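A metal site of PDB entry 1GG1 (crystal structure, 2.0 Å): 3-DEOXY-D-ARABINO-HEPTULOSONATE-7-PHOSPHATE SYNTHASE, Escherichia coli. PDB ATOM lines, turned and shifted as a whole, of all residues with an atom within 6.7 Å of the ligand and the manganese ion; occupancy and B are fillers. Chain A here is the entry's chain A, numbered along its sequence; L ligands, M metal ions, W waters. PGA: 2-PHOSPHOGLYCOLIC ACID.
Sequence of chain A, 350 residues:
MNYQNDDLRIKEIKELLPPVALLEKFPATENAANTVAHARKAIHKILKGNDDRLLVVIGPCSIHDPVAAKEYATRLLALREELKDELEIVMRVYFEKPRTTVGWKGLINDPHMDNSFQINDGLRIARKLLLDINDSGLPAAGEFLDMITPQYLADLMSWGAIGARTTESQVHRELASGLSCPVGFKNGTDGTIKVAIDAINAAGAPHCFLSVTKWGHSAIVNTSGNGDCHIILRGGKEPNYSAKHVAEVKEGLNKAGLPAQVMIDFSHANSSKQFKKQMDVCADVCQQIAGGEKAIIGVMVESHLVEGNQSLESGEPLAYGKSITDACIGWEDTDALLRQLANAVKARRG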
ATOM      1  N   PRO A  60      34.424  12.174  19.178  1.00  0.00           N
ATOM      2  CA  PRO A  60      35.147  12.380  20.430  1.00  0.00           C
ATOM      3  C   PRO A  60      34.283  12.975  21.536  1.00  0.00           C
ATOM      4  O   PRO A  60      33.201  13.545  21.270  1.00  0.00           O
ATOM      5  CB  PRO A  60      36.274  13.323  20.028  1.00  0.00           C
ATOM      6  CG  PRO A  60      36.457  13.047  18.552  1.00  0.00           C
ATOM      7  CD  PRO A  60      35.035  12.974  18.100  1.00  0.00           C
ATOM      8  N   CYS A  61      34.769  12.845  22.772  1.00  0.00           N
ATOM      9  CA  CYS A  61      34.092  13.421  23.931  1.00  0.00           C
ATOM     10  C   CYS A  61      34.164  14.941  23.763  1.00  0.00           C
ATOM     11  O   CYS A  61      33.220  15.651  24.104  1.00  0.00           O
ATOM     12  CB  CYS A  61      34.785  12.969  25.231  1.00  0.00           C
ATOM     13  SG  CYS A  61      34.228  13.793  26.768  1.00  0.00           S
ATOM     14  N   SER A  62      35.266  15.438  23.225  1.00  0.00           N
ATOM     15  CA  SER A  62      35.426  16.881  23.011  1.00  0.00           C
ATOM     16  C   SER A  62      36.475  17.148  21.930  1.00  0.00           C
ATOM     17  O   SER A  62      37.482  16.449  21.868  1.00  0.00           O
ATOM     18  CB  SER A  62      35.879  17.549  24.311  1.00  0.00           C
ATOM     19  OG  SER A  62      37.101  16.988  24.751  1.00  0.00           O
ATOM     20  N   ARG A  92      30.010  13.854  16.428  1.00  0.00           N
ATOM     21  CA  ARG A  92      30.031  14.563  17.712  1.00  0.00           C
ATOM     22  C   ARG A  92      31.128  15.616  17.589  1.00  0.00           C
ATOM     23  O   ARG A  92      32.306  15.290  17.509  1.00  0.00           O
ATOM     24  CB  ARG A  92      30.417  13.649  18.881  1.00  0.00           C
ATOM     25  CG  ARG A  92      29.284  12.808  19.447  1.00  0.00           C
ATOM     26  CD  ARG A  92      29.741  12.006  20.680  1.00  0.00           C
ATOM     27  NE  ARG A  92      30.357  12.874  21.684  1.00  0.00           N
ATOM     28  CZ  ARG A  92      29.932  13.015  22.950  1.00  0.00           C
ATOM     29  NH1 ARG A  92      28.864  12.349  23.399  1.00  0.00           N
ATOM     30  NH2 ARG A  92      30.568  13.816  23.779  1.00  0.00           N
ATOM     31  N   TYR A  94      31.773  18.431  19.871  1.00  0.00           N
ATOM     32  CA  TYR A  94      31.536  19.118  21.135  1.00  0.00           C
ATOM     33  C   TYR A  94      32.609  20.141  21.506  1.00  0.00           C
ATOM     34  O   TYR A  94      33.770  19.789  21.712  1.00  0.00           O
ATOM     35  CB  TYR A  94      31.421  18.101  22.274  1.00  0.00           C
ATOM     36  CG  TYR A  94      30.100  17.347  22.313  1.00  0.00           C
ATOM     37  CD1 TYR A  94      29.523  16.861  21.150  1.00  0.00           C
ATOM     38  CD2 TYR A  94      29.455  17.105  23.533  1.00  0.00           C
ATOM     39  CE1 TYR A  94      28.339  16.145  21.184  1.00  0.00           C
ATOM     40  CE2 TYR A  94      28.264  16.383  23.579  1.00  0.00           C
ATOM     41  CZ  TYR A  94      27.721  15.913  22.401  1.00  0.00           C
ATOM     42  OH  TYR A  94      26.540  15.205  22.433  1.00  0.00           O
ATOM     43  N   LYS A  97      32.315  21.638  27.455  1.00  0.00           N
ATOM     44  CA  LYS A  97      32.256  20.538  28.408  1.00  0.00           C
ATOM     45  C   LYS A  97      31.909  20.965  29.819  1.00  0.00           C
ATOM     46  O   LYS A  97      32.614  21.769  30.430  1.00  0.00           O
ATOM     47  CB  LYS A  97      33.597  19.811  28.443  1.00  0.00           C
ATOM     48  CG  LYS A  97      33.975  19.155  27.120  1.00  0.00           C
ATOM     49  CD  LYS A  97      33.699  17.662  27.119  1.00  0.00           C
ATOM     50  CE  LYS A  97      32.238  17.402  27.013  1.00  0.00           C
ATOM     51  NZ  LYS A  97      31.898  16.040  26.529  1.00  0.00           N
ATOM     52  N   PRO A  98      30.792  20.422  30.369  1.00  0.00           N
ATOM     53  CA  PRO A  98      30.397  20.777  31.732  1.00  0.00           C
ATOM     54  C   PRO A  98      31.260  19.935  32.677  1.00  0.00           C
ATOM     55  O   PRO A  98      31.444  18.734  32.466  1.00  0.00           O
ATOM     56  CB  PRO A  98      28.924  20.373  31.765  1.00  0.00           C
ATOM     57  CG  PRO A  98      28.912  19.134  30.924  1.00  0.00           C
ATOM     58  CD  PRO A  98      29.800  19.530  29.742  1.00  0.00           C
ATOM     59  N   GLU A 143      26.793  19.637  22.421  1.00  0.00           N
ATOM     60  CA  GLU A 143      26.029  19.915  23.623  1.00  0.00           C
ATOM     61  C   GLU A 143      25.846  21.432  23.745  1.00  0.00           C
ATOM     62  O   GLU A 143      26.796  22.207  23.655  1.00  0.00           O
ATOM     63  CB  GLU A 143      26.715  19.402  24.889  1.00  0.00           C
ATOM     64  CG  GLU A 143      25.825  19.701  26.121  1.00  0.00           C
ATOM     65  CD  GLU A 143      26.404  19.278  27.454  1.00  0.00           C
ATOM     66  OE1 GLU A 143      27.198  18.322  27.494  1.00  0.00           O
ATOM     67  OE2 GLU A 143      26.025  19.908  28.483  1.00  0.00           O
ATOM     68  N   ALA A 161      22.547  18.222  22.131  1.00  0.00           N
ATOM     69  CA  ALA A 161      22.313  17.535  23.393  1.00  0.00           C
ATOM     70  C   ALA A 161      22.271  18.486  24.592  1.00  0.00           C
ATOM     71  O   ALA A 161      22.937  19.523  24.606  1.00  0.00           O
ATOM     72  CB  ALA A 161      23.404  16.490  23.621  1.00  0.00           C
ATOM     73  N   ILE A 162      21.441  18.158  25.582  1.00  0.00           N
ATOM     74  CA  ILE A 162      21.388  18.936  26.817  1.00  0.00           C
ATOM     75  C   ILE A 162      21.947  17.934  27.817  1.00  0.00           C
ATOM     76  O   ILE A 162      21.410  16.829  27.969  1.00  0.00           O
ATOM     77  CB  ILE A 162      19.935  19.341  27.258  1.00  0.00           C
ATOM     78  CG1 ILE A 162      19.253  20.261  26.240  1.00  0.00           C
ATOM     79  CG2 ILE A 162      19.924  20.107  28.585  1.00  0.00           C
ATOM     80  CD1 ILE A 162      20.007  21.570  26.000  1.00  0.00           C
ATOM     81  N   GLY A 163      23.039  18.321  28.459  1.00  0.00           N
ATOM     82  CA  GLY A 163      23.695  17.472  29.423  1.00  0.00           C
ATOM     83  C   GLY A 163      22.874  17.039  30.639  1.00  0.00           C
ATOM     84  O   GLY A 163      21.943  17.727  31.077  1.00  0.00           O
ATOM     85  N   ALA A 164      23.239  15.886  31.199  1.00  0.00           N
ATOM     86  CA  ALA A 164      22.539  15.350  32.359  1.00  0.00           C
ATOM     87  C   ALA A 164      22.444  16.348  33.503  1.00  0.00           C
ATOM     88  O   ALA A 164      21.517  16.297  34.332  1.00  0.00           O
ATOM     89  CB  ALA A 164      23.242  14.100  32.849  1.00  0.00           C
ATOM     90  N   ARG A 165      23.410  17.260  33.572  1.00  0.00           N
ATOM     91  CA  ARG A 165      23.489  18.235  34.660  1.00  0.00           C
ATOM     92  C   ARG A 165      22.629  19.450  34.434  1.00  0.00           C
ATOM     93  O   ARG A 165      22.499  20.253  35.343  1.00  0.00           O
ATOM     94  CB  ARG A 165      24.939  18.680  34.904  1.00  0.00           C
ATOM     95  CG  ARG A 165      25.848  17.511  35.319  1.00  0.00           C
ATOM     96  CD  ARG A 165      27.346  17.854  35.300  1.00  0.00           C
ATOM     97  NE  ARG A 165      28.142  16.611  35.417  1.00  0.00           N
ATOM     98  CZ  ARG A 165      28.221  15.664  34.478  1.00  0.00           C
ATOM     99  NH1 ARG A 165      27.566  15.790  33.322  1.00  0.00           N
ATOM    100  NH2 ARG A 165      28.933  14.569  34.706  1.00  0.00           N
ATOM    101  N   THR A 166      22.092  19.586  33.231  1.00  0.00           N
ATOM    102  CA  THR A 166      21.260  20.734  32.881  1.00  0.00           C
ATOM    103  C   THR A 166      19.907  20.353  32.277  1.00  0.00           C
ATOM    104  O   THR A 166      19.141  21.218  31.903  1.00  0.00           O
ATOM    105  CB  THR A 166      21.979  21.662  31.889  1.00  0.00           C
ATOM    106  OG1 THR A 166      22.675  20.896  30.902  1.00  0.00           O
ATOM    107  CG2 THR A 166      22.988  22.559  32.638  1.00  0.00           C
ATOM    108  N   LYS A 186      19.431  14.318  28.143  1.00  0.00           N
ATOM    109  CA  LYS A 186      19.949  13.213  28.913  1.00  0.00           C
ATOM    110  C   LYS A 186      19.232  13.071  30.247  1.00  0.00           C
ATOM    111  O   LYS A 186      18.797  14.071  30.834  1.00  0.00           O
ATOM    112  CB  LYS A 186      21.444  13.420  29.150  1.00  0.00           C
ATOM    113  CG  LYS A 186      22.237  13.374  27.836  1.00  0.00           C
ATOM    114  CD  LYS A 186      23.664  13.016  28.124  1.00  0.00           C
ATOM    115  CE  LYS A 186      24.341  12.293  26.947  1.00  0.00           C
ATOM    116  NZ  LYS A 186      25.677  11.884  27.452  1.00  0.00           N
ATOM    117  N   ASN A 187      19.113  11.843  30.737  1.00  0.00           N
ATOM    118  CA  ASN A 187      18.495  11.644  32.032  1.00  0.00           C
ATOM    119  C   ASN A 187      19.475  12.173  33.080  1.00  0.00           C
ATOM    120  O   ASN A 187      20.659  12.386  32.771  1.00  0.00           O
ATOM    121  CB  ASN A 187      18.152  10.154  32.270  1.00  0.00           C
ATOM    122  CG  ASN A 187      19.387   9.230  32.251  1.00  0.00           C
ATOM    123  OD1 ASN A 187      19.517   8.378  31.363  1.00  0.00           O
ATOM    124  ND2 ASN A 187      20.262   9.365  33.248  1.00  0.00           N
ATOM    125  N   THR A 189      22.067  12.782  36.285  1.00  0.00           N
ATOM    126  CA  THR A 189      23.307  12.073  36.608  1.00  0.00           C
ATOM    127  C   THR A 189      23.065  10.912  37.579  1.00  0.00           C
ATOM    128  O   THR A 189      23.787   9.930  37.551  1.00  0.00           O
ATOM    129  CB  THR A 189      24.386  13.046  37.167  1.00  0.00           C
ATOM    130  OG1 THR A 189      23.855  13.801  38.253  1.00  0.00           O
ATOM    131  CG2 THR A 189      24.882  14.002  36.066  1.00  0.00           C
ATOM    132  N   ARG A 234      21.551   7.589  29.499  1.00  0.00           N
ATOM    133  CA  ARG A 234      22.980   7.620  29.725  1.00  0.00           C
ATOM    134  C   ARG A 234      23.425   7.021  31.041  1.00  0.00           C
ATOM    135  O   ARG A 234      24.560   7.216  31.480  1.00  0.00           O
ATOM    136  CB  ARG A 234      23.503   9.062  29.585  1.00  0.00           C
ATOM    137  CG  ARG A 234      22.761  10.154  30.422  1.00  0.00           C
ATOM    138  CD  ARG A 234      23.267  10.175  31.836  1.00  0.00           C
ATOM    139  NE  ARG A 234      24.620  10.706  31.908  1.00  0.00           N
ATOM    140  CZ  ARG A 234      25.403  10.587  32.975  1.00  0.00           C
ATOM    141  NH1 ARG A 234      24.961   9.954  34.042  1.00  0.00           N
ATOM    142  NH2 ARG A 234      26.620  11.102  32.971  1.00  0.00           N
ATOM    143  N   ASP A 265      22.945   6.208  24.968  1.00  0.00           N
ATOM    144  CA  ASP A 265      24.345   6.602  25.002  1.00  0.00           C
ATOM    145  C   ASP A 265      25.099   5.390  25.497  1.00  0.00           C
ATOM    146  O   ASP A 265      24.908   4.934  26.619  1.00  0.00           O
ATOM    147  CB  ASP A 265      24.517   7.792  25.956  1.00  0.00           C
ATOM    148  CG  ASP A 265      25.939   8.266  26.070  1.00  0.00           C
ATOM    149  OD1 ASP A 265      26.831   7.706  25.407  1.00  0.00           O
ATOM    150  OD2 ASP A 265      26.175   9.219  26.848  1.00  0.00           O
ATOM    151  N   SER A 267      28.091   5.287  26.172  1.00  0.00           N
ATOM    152  CA  SER A 267      29.180   5.709  27.055  1.00  0.00           C
ATOM    153  C   SER A 267      28.771   6.267  28.418  1.00  0.00           C
ATOM    154  O   SER A 267      27.648   6.063  28.878  1.00  0.00           O
ATOM    155  CB  SER A 267      30.037   6.749  26.331  1.00  0.00           C
ATOM    156  OG  SER A 267      31.262   6.951  26.993  1.00  0.00           O
ATOM    157  N   HIS A 268      29.713   6.941  29.071  1.00  0.00           N
ATOM    158  CA  HIS A 268      29.487   7.528  30.383  1.00  0.00           C
ATOM    159  C   HIS A 268      28.986   6.540  31.437  1.00  0.00           C
ATOM    160  O   HIS A 268      29.637   5.527  31.685  1.00  0.00           O
ATOM    161  CB  HIS A 268      28.507   8.706  30.262  1.00  0.00           C
ATOM    162  CG  HIS A 268      28.949   9.746  29.277  1.00  0.00           C
ATOM    163  ND1 HIS A 268      28.460   9.798  27.991  1.00  0.00           N
ATOM    164  CD2 HIS A 268      29.880  10.722  29.373  1.00  0.00           C
ATOM    165  CE1 HIS A 268      29.073  10.755  27.326  1.00  0.00           C
ATOM    166  NE2 HIS A 268      29.944  11.336  28.141  1.00  0.00           N
ATOM    167  N   ALA A 269      27.849   6.844  32.046  1.00  0.00           N
ATOM    168  CA  ALA A 269      27.306   5.992  33.105  1.00  0.00           C
ATOM    169  C   ALA A 269      26.836   4.641  32.609  1.00  0.00           C
ATOM    170  O   ALA A 269      26.695   3.724  33.400  1.00  0.00           O
ATOM    171  CB  ALA A 269      26.174   6.711  33.831  1.00  0.00           C
ATOM    172  N   MET A 300      24.405   6.981  20.848  1.00  0.00           N
ATOM    173  CA  MET A 300      25.457   7.967  20.980  1.00  0.00           C
ATOM    174  C   MET A 300      26.668   7.198  21.446  1.00  0.00           C
ATOM    175  O   MET A 300      26.580   6.388  22.378  1.00  0.00           O
ATOM    176  CB  MET A 300      25.057   9.033  22.011  1.00  0.00           C
ATOM    177  CG  MET A 300      26.160  10.047  22.387  1.00  0.00           C
ATOM    178  SD  MET A 300      25.591  11.282  23.612  1.00  0.00           S
ATOM    179  CE  MET A 300      24.518  12.275  22.582  1.00  0.00           C
ATOM    180  N   GLU A 302      31.169   7.495  22.081  1.00  0.00           N
ATOM    181  CA  GLU A 302      32.374   8.283  22.212  1.00  0.00           C
ATOM    182  C   GLU A 302      33.552   7.542  21.587  1.00  0.00           C
ATOM    183  O   GLU A 302      34.114   6.629  22.199  1.00  0.00           O
ATOM    184  CB  GLU A 302      32.656   8.589  23.689  1.00  0.00           C
ATOM    185  CG  GLU A 302      31.717   9.691  24.226  1.00  0.00           C
ATOM    186  CD  GLU A 302      32.039  10.159  25.626  1.00  0.00           C
ATOM    187  OE1 GLU A 302      32.087  11.395  25.828  1.00  0.00           O
ATOM    188  OE2 GLU A 302      32.223   9.310  26.528  1.00  0.00           O
ATOM    189  N   THR A 325      39.543  14.283  27.377  1.00  0.00           N
ATOM    190  CA  THR A 325      38.477  14.293  28.366  1.00  0.00           C
ATOM    191  C   THR A 325      38.077  12.860  28.777  1.00  0.00           C
ATOM    192  O   THR A 325      38.779  12.233  29.572  1.00  0.00           O
ATOM    193  CB  THR A 325      37.235  15.080  27.879  1.00  0.00           C
ATOM    194  OG1 THR A 325      36.993  14.775  26.502  1.00  0.00           O
ATOM    195  CG2 THR A 325      37.477  16.579  28.015  1.00  0.00           C
ATOM    196  N   ASP A 326      36.962  12.350  28.260  1.00  0.00           N
ATOM    197  CA  ASP A 326      36.545  10.981  28.601  1.00  0.00           C
ATOM    198  C   ASP A 326      37.206  10.026  27.600  1.00  0.00           C
ATOM    199  O   ASP A 326      37.471  10.419  26.467  1.00  0.00           O
ATOM    200  CB  ASP A 326      35.007  10.800  28.522  1.00  0.00           C
ATOM    201  CG  ASP A 326      34.248  11.567  29.633  1.00  0.00           C
ATOM    202  OD1 ASP A 326      34.757  11.700  30.778  1.00  0.00           O
ATOM    203  OD2 ASP A 326      33.102  12.024  29.353  1.00  0.00           O
HETATM  204  P   PGA L   1      26.547  13.771  30.173  1.00  0.00           P
HETATM  205  O1P PGA L   1      27.127  13.698  28.639  1.00  0.00           O
HETATM  206  O2P PGA L   1      27.723  13.704  31.105  1.00  0.00           O
HETATM  207  O3P PGA L   1      25.814  15.084  30.228  1.00  0.00           O
HETATM  208  O4P PGA L   1      25.646  12.571  30.257  1.00  0.00           O
HETATM  209  C2  PGA L   1      28.400  14.268  28.308  1.00  0.00           C
HETATM  210  C1  PGA L   1      28.857  13.964  26.891  1.00  0.00           C
HETATM  211  O1  PGA L   1      28.138  13.720  25.903  1.00  0.00           O
HETATM  212  O2  PGA L   1      30.092  13.924  26.689  1.00  0.00           O
HETATM  213 MN    MN M   1      31.863  12.589  27.628  1.00  0.00          MN
HETATM  214  O   HOH W   1      25.921  14.279  24.990  1.00  0.00           O
HETATM  215  O   HOH W   2      25.719  15.776  27.161  1.00  0.00           O
HETATM  216  O   HOH W   3      29.317  12.759  32.631  1.00  0.00           O
HETATM  217  O   HOH W   4      25.905  17.221  32.038  1.00  0.00           O
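NZ of Lys 186 lies within salt-bridge range of O4P of the ligand, at 2.9 Å. The guanidinium group (NE) of Arg 234 is in salt-bridge range of an oxygen (O4P) of the ligand (2.7 Å). NZ of Lys 97 sits close to O2 of the ligand. N of Ala 164 lies within hydrogen-bond range of O3P of the ligand (2.9 Å). An oxygen (O1) of the ligand lies within salt-bridge range of the guanidinium group of Arg 92, 2.9 Å away. The guanidinium group (NH1) of Arg 165 is in salt-bridge range of an oxygen (O2P) of the ligand.
Residues that only touch the manganese ion: Lys 97 (3.6 Å). Of the 26 residues printed, 5 come within 4 Å of the manganese ion. The nearest printed residue that does not touch the manganese ion is Arg 92 (4.2 Å).
The manganese ion is bound by OE1 of Glu 302, at 2.2 Å. The side-chain carboxylate (OD2) of Asp 326 is bound to the manganese ion, 2.2 Å away. The manganese ion is bound by NE2 of His 268 (2.3 Å). O2 of the ligand binds the manganese ion (2.4 Å). The manganese ion is bound by the side-chain sulfur (SG) of Cys 61 (2.8 Å).
Merely in contact with the ligand: Tyr 94 (3.5 Å) and Gly 163 (3.3 Å). Ten residues have an atom within 4 Å of the ligand: Arg 92, Tyr 94, Lys 97, Gly 163, Ala 164, Arg 165, Lys 186, Arg 234, His 268 and Glu 302. The nearest printed residue that does not touch the ligand is Cys 61 (4.1 Å).
Water W3 lies within hydrogen-bond range of O2P of the ligand (2.4 Å), NH2 of Arg 165 (2.8 Å) and NH2 of Arg 234 (3.2 Å). Water W1 lies within hydrogen-bond range of O1 of the ligand (2.5 Å), OH of Tyr 94 (2.8 Å), SD of Met 300 (3.3 Å) and NZ of Lys 186 (3.4 Å). Water W4 lies within hydrogen-bond range of the guanidinium group (NH1) of Arg 165 (2.5 Å), an oxygen (O3P) of the ligand (2.8 Å) and the backbone NH (N) of Ala 164 (3.1 Å). Water W2 lies within hydrogen-bond range of O1P of the ligand (2.9 Å) and OE1 of Glu 143 (3.0 Å).
The side-chain carboxylate (OD2) of Asp 265 lies within hydrogen-bond range of a ring nitrogen (ND1) of His 268 (2.6 Å). The side-chain amino group of Lys 186 lies within salt-bridge range of the side-chain carboxylate of Asp 265, at 2.8 Å. The backbone NH (N) of Arg 234 lies within hydrogen-bond range of the side-chain amide oxygen (OD1) of Asn 187. N of Ala 269 sits close to O of Arg 234, at 3.4 Å. The side-chain amino group (NZ) of Lys 97 sits at hydrogen-bond distance from the backbone carbonyl oxygen (O) of Cys 61 (2.8 Å). The guanidinium group of Arg 92 lies within hydrogen-bond range of the backbone carbonyl oxygen of Cys 61 (3.2 Å). O of Pro 60 lies within hydrogen-bond range of NE of Arg 92, 3.0 Å away. OG1 of Thr 166 is in hydrogen-bond range of O of Gly 163 (3.3 Å).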
